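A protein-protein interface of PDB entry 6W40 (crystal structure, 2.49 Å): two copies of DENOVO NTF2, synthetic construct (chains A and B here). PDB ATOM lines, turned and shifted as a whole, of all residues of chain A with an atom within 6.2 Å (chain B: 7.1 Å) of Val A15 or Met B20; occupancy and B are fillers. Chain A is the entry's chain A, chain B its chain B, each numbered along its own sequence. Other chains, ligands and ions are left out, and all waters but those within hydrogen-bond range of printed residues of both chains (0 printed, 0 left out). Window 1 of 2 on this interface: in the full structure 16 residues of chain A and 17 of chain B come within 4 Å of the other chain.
SD of Met A20 sits close to N of Asn B69 (3.3 Å).
OE1 of Glu B13 lies close to SD of Met A11, at 3.2 Å.
SD of Met A12 sits close to N of Ile B72, at 3.6 Å.
OG1 of Thr B21 sits at hydrogen-bond distance from O of Asp B23 (2.9 Å).
O of Glu B13 sits at hydrogen-bond distance from NZ of Lys B17, at 2.9 Å.
O of Asn B69 lies within hydrogen-bond range of NE of Arg B71.
The backbone carbonyl oxygen of Val A15 sits at hydrogen-bond distance from the backbone NH of Met A20, 2.5 Å away.
Among the printed residues, pairs that only touch across the chains: Met A12 with Ile B70 (3.8 Å), Ile A14 with Lys B17 (3.7 Å), Val A15 with Met B20 (3.8 Å), Leu A18 with Met B20 (3.7 Å), Phe A19 with Met B20 (3.4 Å), Phe A19 with Ile B70 (3.7 Å), Met A20 with Ile B70 (3.4 Å), Ile A72 with Met B20 (3.2 Å), Ile A72 with Thr B21 (3.8 Å) and Ile A75 with Lys B17 (3.6 Å).
Val A15 touches just one residue of chain B: Met B20 (3.8 Å).
Of the printed residues of chain B, Ile A72 touches Met B20 (3.2 Å) and Thr B21 (3.8 Å).
Of the printed residues of chain A, Glu B13 touches Met A11.
Met B20 touches four residues of chain A.
Gly B22 touches none of the printed residues of chain A.
Asp B23 touches none of the printed residues of chain A.
Of the printed residues of chain A, Ile B70 touches Met A12, Phe A19 and Met A20.
Of the printed residues of chain A, Ile B72 touches Met A12.
The nearest residue of chain A that does not touch Met B20 is Ile A14 (4.1 Å).
The nearest printed residue of chain A that does not touch Lys B17 is Met A11 (4.3 Å).
Of the 16 printed residues of chain A, 9 touch a printed residue of chain B.
Hydrophobic or aromatic side chains of chain A within 4 Å of the printed part of chain B: Met A11, Met A12, Ile A14, Val A15, Phe A19, Met A20, Ile A72 and Ile A75.
Along chain A the printed residues that touch a printed residue of chain B span positions 11 to 75.
Among the printed residues, 13 pairs touch across the chains.
Among the printed residues, no Asp or Glu carboxylate lies within 4 Å of a Lys or Arg side-chain nitrogen of the other chain.
Leu A18 touches Met B20, but with the chains exchanged Met A20 does not touch Leu B18 (11.3 Å).
Met A20 touches Ile B70, but with the chains exchanged Ile A70 does not touch Met B20 (5.4 Å).
Ile A72 touches Met B20, but with the chains exchanged Met A20 does not touch Ile B72 (9.1 Å).
Ile A72 touches Thr B21, but with the chains exchanged Thr A21 does not touch Ile B72 (13.8 Å).
10 positions are printed for both chains.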
ATOM      1  N   ASP A  10      -4.031  -7.679  32.358  1.00  0.00           N
ATOM      2  CA  ASP A  10      -3.005  -7.351  31.372  1.00  0.00           C
ATOM      3  C   ASP A  10      -1.797  -8.272  31.506  1.00  0.00           C
ATOM      4  O   ASP A  10      -1.309  -8.823  30.513  1.00  0.00           O
ATOM      5  CB  ASP A  10      -2.586  -5.887  31.519  1.00  0.00           C
ATOM      6  CG  ASP A  10      -3.103  -5.012  30.390  1.00  0.00           C
ATOM      7  OD1 ASP A  10      -3.195  -5.504  29.246  1.00  0.00           O
ATOM      8  OD2 ASP A  10      -3.414  -3.829  30.643  1.00  0.00           O
ATOM      9  N   MET A  11      -1.308  -8.460  32.736  1.00  0.00           N
ATOM     10  CA  MET A  11      -0.142  -9.311  32.957  1.00  0.00           C
ATOM     11  C   MET A  11      -0.405 -10.746  32.517  1.00  0.00           C
ATOM     12  O   MET A  11       0.461 -11.384  31.906  1.00  0.00           O
ATOM     13  CB  MET A  11       0.267  -9.274  34.429  1.00  0.00           C
ATOM     14  CG  MET A  11       1.043  -8.034  34.830  1.00  0.00           C
ATOM     15  SD  MET A  11       2.696  -8.003  34.109  1.00  0.00           S
ATOM     16  CE  MET A  11       3.398  -9.494  34.812  1.00  0.00           C
ATOM     17  N   MET A  12      -1.593 -11.275  32.822  1.00  0.00           N
ATOM     18  CA  MET A  12      -1.923 -12.633  32.404  1.00  0.00           C
ATOM     19  C   MET A  12      -1.958 -12.763  30.886  1.00  0.00           C
ATOM     20  O   MET A  12      -1.669 -13.839  30.349  1.00  0.00           O
ATOM     21  CB  MET A  12      -3.260 -13.065  33.008  1.00  0.00           C
ATOM     22  CG  MET A  12      -3.158 -13.559  34.442  1.00  0.00           C
ATOM     23  SD  MET A  12      -4.747 -14.021  35.160  1.00  0.00           S
ATOM     24  CE  MET A  12      -5.355 -15.175  33.931  1.00  0.00           C
ATOM     25  N   GLU A  13      -2.309 -11.688  30.177  1.00  0.00           N
ATOM     26  CA  GLU A  13      -2.248 -11.725  28.720  1.00  0.00           C
ATOM     27  C   GLU A  13      -0.805 -11.817  28.241  1.00  0.00           C
ATOM     28  O   GLU A  13      -0.486 -12.616  27.354  1.00  0.00           O
ATOM     29  CB  GLU A  13      -2.930 -10.492  28.122  1.00  0.00           C
ATOM     30  CG  GLU A  13      -4.346 -10.225  28.612  1.00  0.00           C
ATOM     31  CD  GLU A  13      -5.378 -11.167  28.028  1.00  0.00           C
ATOM     32  OE1 GLU A  13      -5.002 -12.086  27.272  1.00  0.00           O
ATOM     33  OE2 GLU A  13      -6.578 -10.982  28.325  1.00  0.00           O
ATOM     34  N   ILE A  14       0.085 -11.015  28.831  1.00  0.00           N
ATOM     35  CA  ILE A  14       1.471 -10.964  28.370  1.00  0.00           C
ATOM     36  C   ILE A  14       2.143 -12.319  28.532  1.00  0.00           C
ATOM     37  O   ILE A  14       2.862 -12.784  27.640  1.00  0.00           O
ATOM     38  CB  ILE A  14       2.248  -9.866  29.121  1.00  0.00           C
ATOM     39  CG1 ILE A  14       1.447  -8.566  29.168  1.00  0.00           C
ATOM     40  CG2 ILE A  14       3.604  -9.636  28.472  1.00  0.00           C
ATOM     41  CD1 ILE A  14       0.983  -8.076  27.827  1.00  0.00           C
ATOM     42  N   VAL A  15       1.921 -12.975  29.675  1.00  0.00           N
ATOM     43  CA  VAL A  15       2.615 -14.227  29.945  1.00  0.00           C
ATOM     44  C   VAL A  15       2.118 -15.337  29.025  1.00  0.00           C
ATOM     45  O   VAL A  15       2.896 -16.210  28.624  1.00  0.00           O
ATOM     46  CB  VAL A  15       2.478 -14.608  31.434  1.00  0.00           C
ATOM     47  CG1 VAL A  15       3.075 -13.517  32.320  1.00  0.00           C
ATOM     48  CG2 VAL A  15       1.023 -14.854  31.797  1.00  0.00           C
ATOM     49  N   ILE A  16       0.833 -15.320  28.656  1.00  0.00           N
ATOM     50  CA  ILE A  16       0.309 -16.383  27.804  1.00  0.00           C
ATOM     51  C   ILE A  16       0.809 -16.218  26.377  1.00  0.00           C
ATOM     52  O   ILE A  16       1.237 -17.187  25.738  1.00  0.00           O
ATOM     53  CB  ILE A  16      -1.230 -16.421  27.859  1.00  0.00           C
ATOM     54  CG1 ILE A  16      -1.704 -16.942  29.218  1.00  0.00           C
ATOM     55  CG2 ILE A  16      -1.780 -17.287  26.732  1.00  0.00           C
ATOM     56  CD1 ILE A  16      -3.057 -17.643  29.180  1.00  0.00           C
ATOM     57  N   LYS A  17       0.780 -14.989  25.858  1.00  0.00           N
ATOM     58  CA  LYS A  17       1.151 -14.756  24.467  1.00  0.00           C
ATOM     59  C   LYS A  17       2.660 -14.829  24.266  1.00  0.00           C
ATOM     60  O   LYS A  17       3.141 -15.564  23.397  1.00  0.00           O
ATOM     61  CB  LYS A  17       0.630 -13.394  24.003  1.00  0.00           C
ATOM     62  CG  LYS A  17      -0.812 -13.117  24.363  1.00  0.00           C
ATOM     63  CD  LYS A  17      -1.745 -14.143  23.763  1.00  0.00           C
ATOM     64  CE  LYS A  17      -1.814 -13.997  22.263  1.00  0.00           C
ATOM     65  NZ  LYS A  17      -2.101 -12.591  21.874  1.00  0.00           N
ATOM     66  N   LEU A  18       3.419 -14.074  25.060  1.00  0.00           N
ATOM     67  CA  LEU A  18       4.827 -13.824  24.781  1.00  0.00           C
ATOM     68  C   LEU A  18       5.771 -14.506  25.764  1.00  0.00           C
ATOM     69  O   LEU A  18       6.975 -14.232  25.737  1.00  0.00           O
ATOM     70  CB  LEU A  18       5.086 -12.317  24.762  1.00  0.00           C
ATOM     71  CG  LEU A  18       4.155 -11.512  23.850  1.00  0.00           C
ATOM     72  CD1 LEU A  18       3.540 -10.342  24.602  1.00  0.00           C
ATOM     73  CD2 LEU A  18       4.885 -11.026  22.607  1.00  0.00           C
ATOM     74  N   PHE A  19       5.264 -15.387  26.626  1.00  0.00           N
ATOM     75  CA  PHE A  19       6.110 -16.107  27.572  1.00  0.00           C
ATOM     76  C   PHE A  19       5.772 -17.591  27.565  1.00  0.00           C
ATOM     77  O   PHE A  19       6.500 -18.393  26.972  1.00  0.00           O
ATOM     78  CB  PHE A  19       5.951 -15.535  28.983  1.00  0.00           C
ATOM     79  CG  PHE A  19       6.753 -16.255  30.039  1.00  0.00           C
ATOM     80  CD1 PHE A  19       6.350 -16.220  31.364  1.00  0.00           C
ATOM     81  CD2 PHE A  19       7.914 -16.943  29.719  1.00  0.00           C
ATOM     82  CE1 PHE A  19       7.073 -16.871  32.342  1.00  0.00           C
ATOM     83  CE2 PHE A  19       8.640 -17.599  30.694  1.00  0.00           C
ATOM     84  CZ  PHE A  19       8.219 -17.559  32.007  1.00  0.00           C
ATOM     85  N   MET A  20       4.682 -17.959  28.243  1.00  0.00           N
ATOM     86  CA  MET A  20       4.218 -19.339  28.314  1.00  0.00           C
ATOM     87  C   MET A  20       4.186 -19.962  26.925  1.00  0.00           C
ATOM     88  O   MET A  20       3.176 -19.864  26.220  1.00  0.00           O
ATOM     89  CB  MET A  20       2.834 -19.397  28.961  1.00  0.00           C
ATOM     90  CG  MET A  20       2.265 -20.794  29.110  1.00  0.00           C
ATOM     91  SD  MET A  20       0.494 -20.766  29.431  1.00  0.00           S
ATOM     92  CE  MET A  20       0.408 -19.433  30.625  1.00  0.00           C
ATOM     93  N   THR A  21       5.291 -20.623  26.553  1.00  0.00           N
ATOM     94  CA  THR A  21       5.620 -21.031  25.187  1.00  0.00           C
ATOM     95  C   THR A  21       4.992 -20.088  24.165  1.00  0.00           C
ATOM     96  O   THR A  21       5.063 -18.864  24.321  1.00  0.00           O
ATOM     97  CB  THR A  21       5.208 -22.490  24.928  1.00  0.00           C
ATOM     98  OG1 THR A  21       5.355 -22.792  23.534  1.00  0.00           O
ATOM     99  CG2 THR A  21       3.768 -22.781  25.371  1.00  0.00           C
ATOM    100  N   GLY A  22       4.393 -20.633  23.114  1.00  0.00           N
ATOM    101  CA  GLY A  22       3.571 -19.816  22.251  1.00  0.00           C
ATOM    102  C   GLY A  22       2.191 -19.682  22.853  1.00  0.00           C
ATOM    103  O   GLY A  22       1.735 -18.577  23.160  1.00  0.00           O
ATOM    104  N   ILE A  70       7.687 -15.009  20.056  1.00  0.00           N
ATOM    105  CA  ILE A  70       8.148 -13.711  19.577  1.00  0.00           C
ATOM    106  C   ILE A  70       9.365 -13.310  20.400  1.00  0.00           C
ATOM    107  O   ILE A  70       9.243 -13.028  21.599  1.00  0.00           O
ATOM    108  CB  ILE A  70       7.053 -12.640  19.671  1.00  0.00           C
ATOM    109  CG1 ILE A  70       5.828 -13.060  18.860  1.00  0.00           C
ATOM    110  CG2 ILE A  70       7.577 -11.294  19.189  1.00  0.00           C
ATOM    111  CD1 ILE A  70       4.633 -12.167  19.064  1.00  0.00           C
ATOM    112  N   ILE A  72      11.364 -10.903  21.889  1.00  0.00           N
ATOM    113  CA  ILE A  72      10.961  -9.540  22.215  1.00  0.00           C
ATOM    114  C   ILE A  72      12.189  -8.645  22.312  1.00  0.00           C
ATOM    115  O   ILE A  72      13.182  -8.997  22.959  1.00  0.00           O
ATOM    116  CB  ILE A  72      10.158  -9.519  23.525  1.00  0.00           C
ATOM    117  CG1 ILE A  72       8.837 -10.266  23.340  1.00  0.00           C
ATOM    118  CG2 ILE A  72       9.919  -8.091  23.985  1.00  0.00           C
ATOM    119  CD1 ILE A  72       8.043 -10.405  24.606  1.00  0.00           C
ATOM    120  N   ILE A  75       9.095  -3.593  25.023  1.00  0.00           N
ATOM    121  CA  ILE A  75       7.678  -3.639  25.366  1.00  0.00           C
ATOM    122  C   ILE A  75       7.330  -2.392  26.165  1.00  0.00           C
ATOM    123  O   ILE A  75       8.075  -1.986  27.062  1.00  0.00           O
ATOM    124  CB  ILE A  75       7.319  -4.910  26.165  1.00  0.00           C
ATOM    125  CG1 ILE A  75       7.282  -6.131  25.250  1.00  0.00           C
ATOM    126  CG2 ILE A  75       5.980  -4.754  26.861  1.00  0.00           C
ATOM    127  CD1 ILE A  75       6.743  -7.372  25.928  1.00  0.00           C
ATOM    128  N   GLU B  13       6.353  -2.572  36.034  1.00  0.00           N
ATOM    129  CA  GLU B  13       5.725  -3.696  35.348  1.00  0.00           C
ATOM    130  C   GLU B  13       6.482  -4.061  34.080  1.00  0.00           C
ATOM    131  O   GLU B  13       6.687  -5.247  33.794  1.00  0.00           O
ATOM    132  CB  GLU B  13       4.271  -3.363  35.028  1.00  0.00           C
ATOM    133  CG  GLU B  13       3.407  -3.214  36.260  1.00  0.00           C
ATOM    134  CD  GLU B  13       2.949  -4.543  36.811  1.00  0.00           C
ATOM    135  OE1 GLU B  13       2.607  -5.433  36.005  1.00  0.00           O
ATOM    136  OE2 GLU B  13       2.934  -4.702  38.051  1.00  0.00           O
ATOM    137  N   ILE B  16       9.437  -6.143  34.902  1.00  0.00           N
ATOM    138  CA  ILE B  16       9.156  -7.550  35.179  1.00  0.00           C
ATOM    139  C   ILE B  16       9.003  -8.330  33.883  1.00  0.00           C
ATOM    140  O   ILE B  16       9.421  -9.490  33.787  1.00  0.00           O
ATOM    141  CB  ILE B  16       7.905  -7.683  36.064  1.00  0.00           C
ATOM    142  CG1 ILE B  16       8.091  -6.885  37.350  1.00  0.00           C
ATOM    143  CG2 ILE B  16       7.630  -9.141  36.390  1.00  0.00           C
ATOM    144  CD1 ILE B  16       9.386  -7.177  38.054  1.00  0.00           C
ATOM    145  N   LYS B  17       8.420  -7.706  32.862  1.00  0.00           N
ATOM    146  CA  LYS B  17       8.193  -8.390  31.596  1.00  0.00           C
ATOM    147  C   LYS B  17       9.480  -8.712  30.849  1.00  0.00           C
ATOM    148  O   LYS B  17       9.409  -9.282  29.755  1.00  0.00           O
ATOM    149  CB  LYS B  17       7.257  -7.556  30.719  1.00  0.00           C
ATOM    150  CG  LYS B  17       5.832  -7.500  31.254  1.00  0.00           C
ATOM    151  CD  LYS B  17       4.900  -6.751  30.318  1.00  0.00           C
ATOM    152  CE  LYS B  17       5.197  -5.263  30.308  1.00  0.00           C
ATOM    153  NZ  LYS B  17       4.904  -4.621  31.619  1.00  0.00           N
ATOM    154  N   LEU B  18      10.645  -8.374  31.399  1.00  0.00           N
ATOM    155  CA  LEU B  18      11.906  -8.860  30.858  1.00  0.00           C
ATOM    156  C   LEU B  18      12.270 -10.246  31.383  1.00  0.00           C
ATOM    157  O   LEU B  18      13.394 -10.708  31.157  1.00  0.00           O
ATOM    158  CB  LEU B  18      13.030  -7.863  31.150  1.00  0.00           C
ATOM    159  CG  LEU B  18      13.000  -6.554  30.344  1.00  0.00           C
ATOM    160  CD1 LEU B  18      12.399  -6.752  28.964  1.00  0.00           C
ATOM    161  CD2 LEU B  18      12.268  -5.461  31.076  1.00  0.00           C
ATOM    162  N   PHE B  19      11.345 -10.907  32.083  1.00  0.00           N
ATOM    163  CA  PHE B  19      11.410 -12.342  32.341  1.00  0.00           C
ATOM    164  C   PHE B  19      11.102 -13.169  31.102  1.00  0.00           C
ATOM    165  O   PHE B  19      11.171 -14.402  31.165  1.00  0.00           O
ATOM    166  CB  PHE B  19      10.420 -12.733  33.444  1.00  0.00           C
ATOM    167  CG  PHE B  19      11.000 -12.716  34.826  1.00  0.00           C
ATOM    168  CD1 PHE B  19      11.833 -13.736  35.254  1.00  0.00           C
ATOM    169  CD2 PHE B  19      10.686 -11.699  35.711  1.00  0.00           C
ATOM    170  CE1 PHE B  19      12.358 -13.731  36.532  1.00  0.00           C
ATOM    171  CE2 PHE B  19      11.208 -11.687  36.990  1.00  0.00           C
ATOM    172  CZ  PHE B  19      12.045 -12.705  37.400  1.00  0.00           C
ATOM    173  N   MET B  20      10.758 -12.521  29.986  1.00  0.00           N
ATOM    174  CA  MET B  20      10.189 -13.178  28.819  1.00  0.00           C
ATOM    175  C   MET B  20      10.621 -12.419  27.561  1.00  0.00           C
ATOM    176  O   MET B  20       9.827 -11.799  26.857  1.00  0.00           O
ATOM    177  CB  MET B  20       8.666 -13.256  28.933  1.00  0.00           C
ATOM    178  CG  MET B  20       8.068 -12.196  29.853  1.00  0.00           C
ATOM    179  SD  MET B  20       6.274 -12.285  30.017  1.00  0.00           S
ATOM    180  CE  MET B  20       6.002 -11.286  31.476  1.00  0.00           C
ATOM    181  N   THR B  21      11.922 -12.465  27.264  1.00  0.00           N
ATOM    182  CA  THR B  21      12.466 -11.851  26.057  1.00  0.00           C
ATOM    183  C   THR B  21      13.374 -12.819  25.311  1.00  0.00           C
ATOM    184  O   THR B  21      14.298 -12.398  24.609  1.00  0.00           O
ATOM    185  CB  THR B  21      13.219 -10.561  26.379  1.00  0.00           C
ATOM    186  OG1 THR B  21      14.198 -10.816  27.394  1.00  0.00           O
ATOM    187  CG2 THR B  21      12.258  -9.493  26.859  1.00  0.00           C
ATOM    188  N   GLY B  22      13.130 -14.117  25.458  1.00  0.00           N
ATOM    189  CA  GLY B  22      13.944 -15.116  24.795  1.00  0.00           C
ATOM    190  C   GLY B  22      15.307 -15.288  25.431  1.00  0.00           C
ATOM    191  O   GLY B  22      15.684 -16.397  25.820  1.00  0.00           O
ATOM    192  N   ASP B  23      16.056 -14.194  25.544  1.00  0.00           N
ATOM    193  CA  ASP B  23      17.388 -14.206  26.121  1.00  0.00           C
ATOM    194  C   ASP B  23      17.447 -13.244  27.301  1.00  0.00           C
ATOM    195  O   ASP B  23      16.583 -12.379  27.469  1.00  0.00           O
ATOM    196  CB  ASP B  23      18.446 -13.831  25.074  1.00  0.00           C
ATOM    197  CG  ASP B  23      19.762 -14.548  25.291  1.00  0.00           C
ATOM    198  OD1 ASP B  23      19.894 -15.257  26.311  1.00  0.00           O
ATOM    199  OD2 ASP B  23      20.664 -14.410  24.437  1.00  0.00           O
ATOM    200  N   TRP B  24      18.485 -13.406  28.126  1.00  0.00           N
ATOM    201  CA  TRP B  24      18.685 -12.570  29.304  1.00  0.00           C
ATOM    202  C   TRP B  24      19.463 -11.296  28.997  1.00  0.00           C
ATOM    203  O   TRP B  24      20.125 -10.747  29.889  1.00  0.00           O
ATOM    204  CB  TRP B  24      19.386 -13.367  30.406  1.00  0.00           C
ATOM    205  CG  TRP B  24      18.652 -14.610  30.801  1.00  0.00           C
ATOM    206  CD1 TRP B  24      19.042 -15.897  30.576  1.00  0.00           C
ATOM    207  CD2 TRP B  24      17.394 -14.685  31.482  1.00  0.00           C
ATOM    208  NE1 TRP B  24      18.109 -16.770  31.080  1.00  0.00           N
ATOM    209  CE2 TRP B  24      17.086 -16.051  31.641  1.00  0.00           C
ATOM    210  CE3 TRP B  24      16.499 -13.730  31.976  1.00  0.00           C
ATOM    211  CZ2 TRP B  24      15.921 -16.486  32.271  1.00  0.00           C
ATOM    212  CZ3 TRP B  24      15.344 -14.164  32.601  1.00  0.00           C
ATOM    213  CH2 TRP B  24      15.066 -15.530  32.742  1.00  0.00           C
ATOM    214  N   LEU B  62      15.258 -21.145  34.871  1.00  0.00           N
ATOM    215  CA  LEU B  62      14.045 -20.805  34.134  1.00  0.00           C
ATOM    216  C   LEU B  62      13.869 -21.663  32.887  1.00  0.00           C
ATOM    217  O   LEU B  62      12.732 -21.942  32.487  1.00  0.00           O
ATOM    218  CB  LEU B  62      14.062 -19.320  33.763  1.00  0.00           C
ATOM    219  CG  LEU B  62      12.765 -18.642  33.304  1.00  0.00           C
ATOM    220  CD1 LEU B  62      12.543 -18.779  31.802  1.00  0.00           C
ATOM    221  CD2 LEU B  62      11.571 -19.185  34.078  1.00  0.00           C
ATOM    222  N   ASN B  69      -0.044 -22.103  32.451  1.00  0.00           N
ATOM    223  CA  ASN B  69      -1.236 -21.557  33.100  1.00  0.00           C
ATOM    224  C   ASN B  69      -0.857 -20.653  34.273  1.00  0.00           C
ATOM    225  O   ASN B  69      -1.164 -20.922  35.438  1.00  0.00           O
ATOM    226  CB  ASN B  69      -2.176 -22.682  33.544  1.00  0.00           C
ATOM    227  CG  ASN B  69      -3.531 -22.168  33.987  1.00  0.00           C
ATOM    228  OD1 ASN B  69      -3.897 -21.026  33.705  1.00  0.00           O
ATOM    229  ND2 ASN B  69      -4.287 -23.010  34.682  1.00  0.00           N
ATOM    230  N   ILE B  70      -0.169 -19.565  33.943  1.00  0.00           N
ATOM    231  CA  ILE B  70       0.257 -18.594  34.945  1.00  0.00           C
ATOM    232  C   ILE B  70      -0.903 -17.652  35.235  1.00  0.00           C
ATOM    233  O   ILE B  70      -1.414 -16.979  34.334  1.00  0.00           O
ATOM    234  CB  ILE B  70       1.497 -17.819  34.479  1.00  0.00           C
ATOM    235  CG1 ILE B  70       2.667 -18.779  34.251  1.00  0.00           C
ATOM    236  CG2 ILE B  70       1.868 -16.751  35.498  1.00  0.00           C
ATOM    237  CD1 ILE B  70       3.947 -18.095  33.818  1.00  0.00           C
ATOM    238  N   ARG B  71      -1.324 -17.606  36.497  1.00  0.00           N
ATOM    239  CA  ARG B  71      -2.443 -16.786  36.934  1.00  0.00           C
ATOM    240  C   ARG B  71      -1.940 -15.755  37.932  1.00  0.00           C
ATOM    241  O   ARG B  71      -1.176 -16.093  38.842  1.00  0.00           O
ATOM    242  CB  ARG B  71      -3.537 -17.654  37.560  1.00  0.00           C
ATOM    243  CG  ARG B  71      -4.190 -18.622  36.584  1.00  0.00           C
ATOM    244  CD  ARG B  71      -4.453 -19.974  37.232  1.00  0.00           C
ATOM    245  NE  ARG B  71      -3.241 -20.786  37.321  1.00  0.00           N
ATOM    246  CZ  ARG B  71      -3.176 -21.975  37.914  1.00  0.00           C
ATOM    247  NH1 ARG B  71      -4.256 -22.497  38.481  1.00  0.00           N
ATOM    248  NH2 ARG B  71      -2.031 -22.643  37.944  1.00  0.00           N
ATOM    249  N   ILE B  72      -2.364 -14.506  37.763  1.00  0.00           N
ATOM    250  CA  ILE B  72      -1.943 -13.406  38.623  1.00  0.00           C
ATOM    251  C   ILE B  72      -3.073 -13.097  39.597  1.00  0.00           C
ATOM    252  O   ILE B  72      -4.190 -12.767  39.181  1.00  0.00           O
ATOM    253  CB  ILE B  72      -1.559 -12.165  37.801  1.00  0.00           C
ATOM    254  CG1 ILE B  72      -0.545 -12.537  36.719  1.00  0.00           C
ATOM    255  CG2 ILE B  72      -0.983 -11.086  38.706  1.00  0.00           C
ATOM    256  CD1 ILE B  72       0.735 -13.140  37.259  1.00  0.00           C
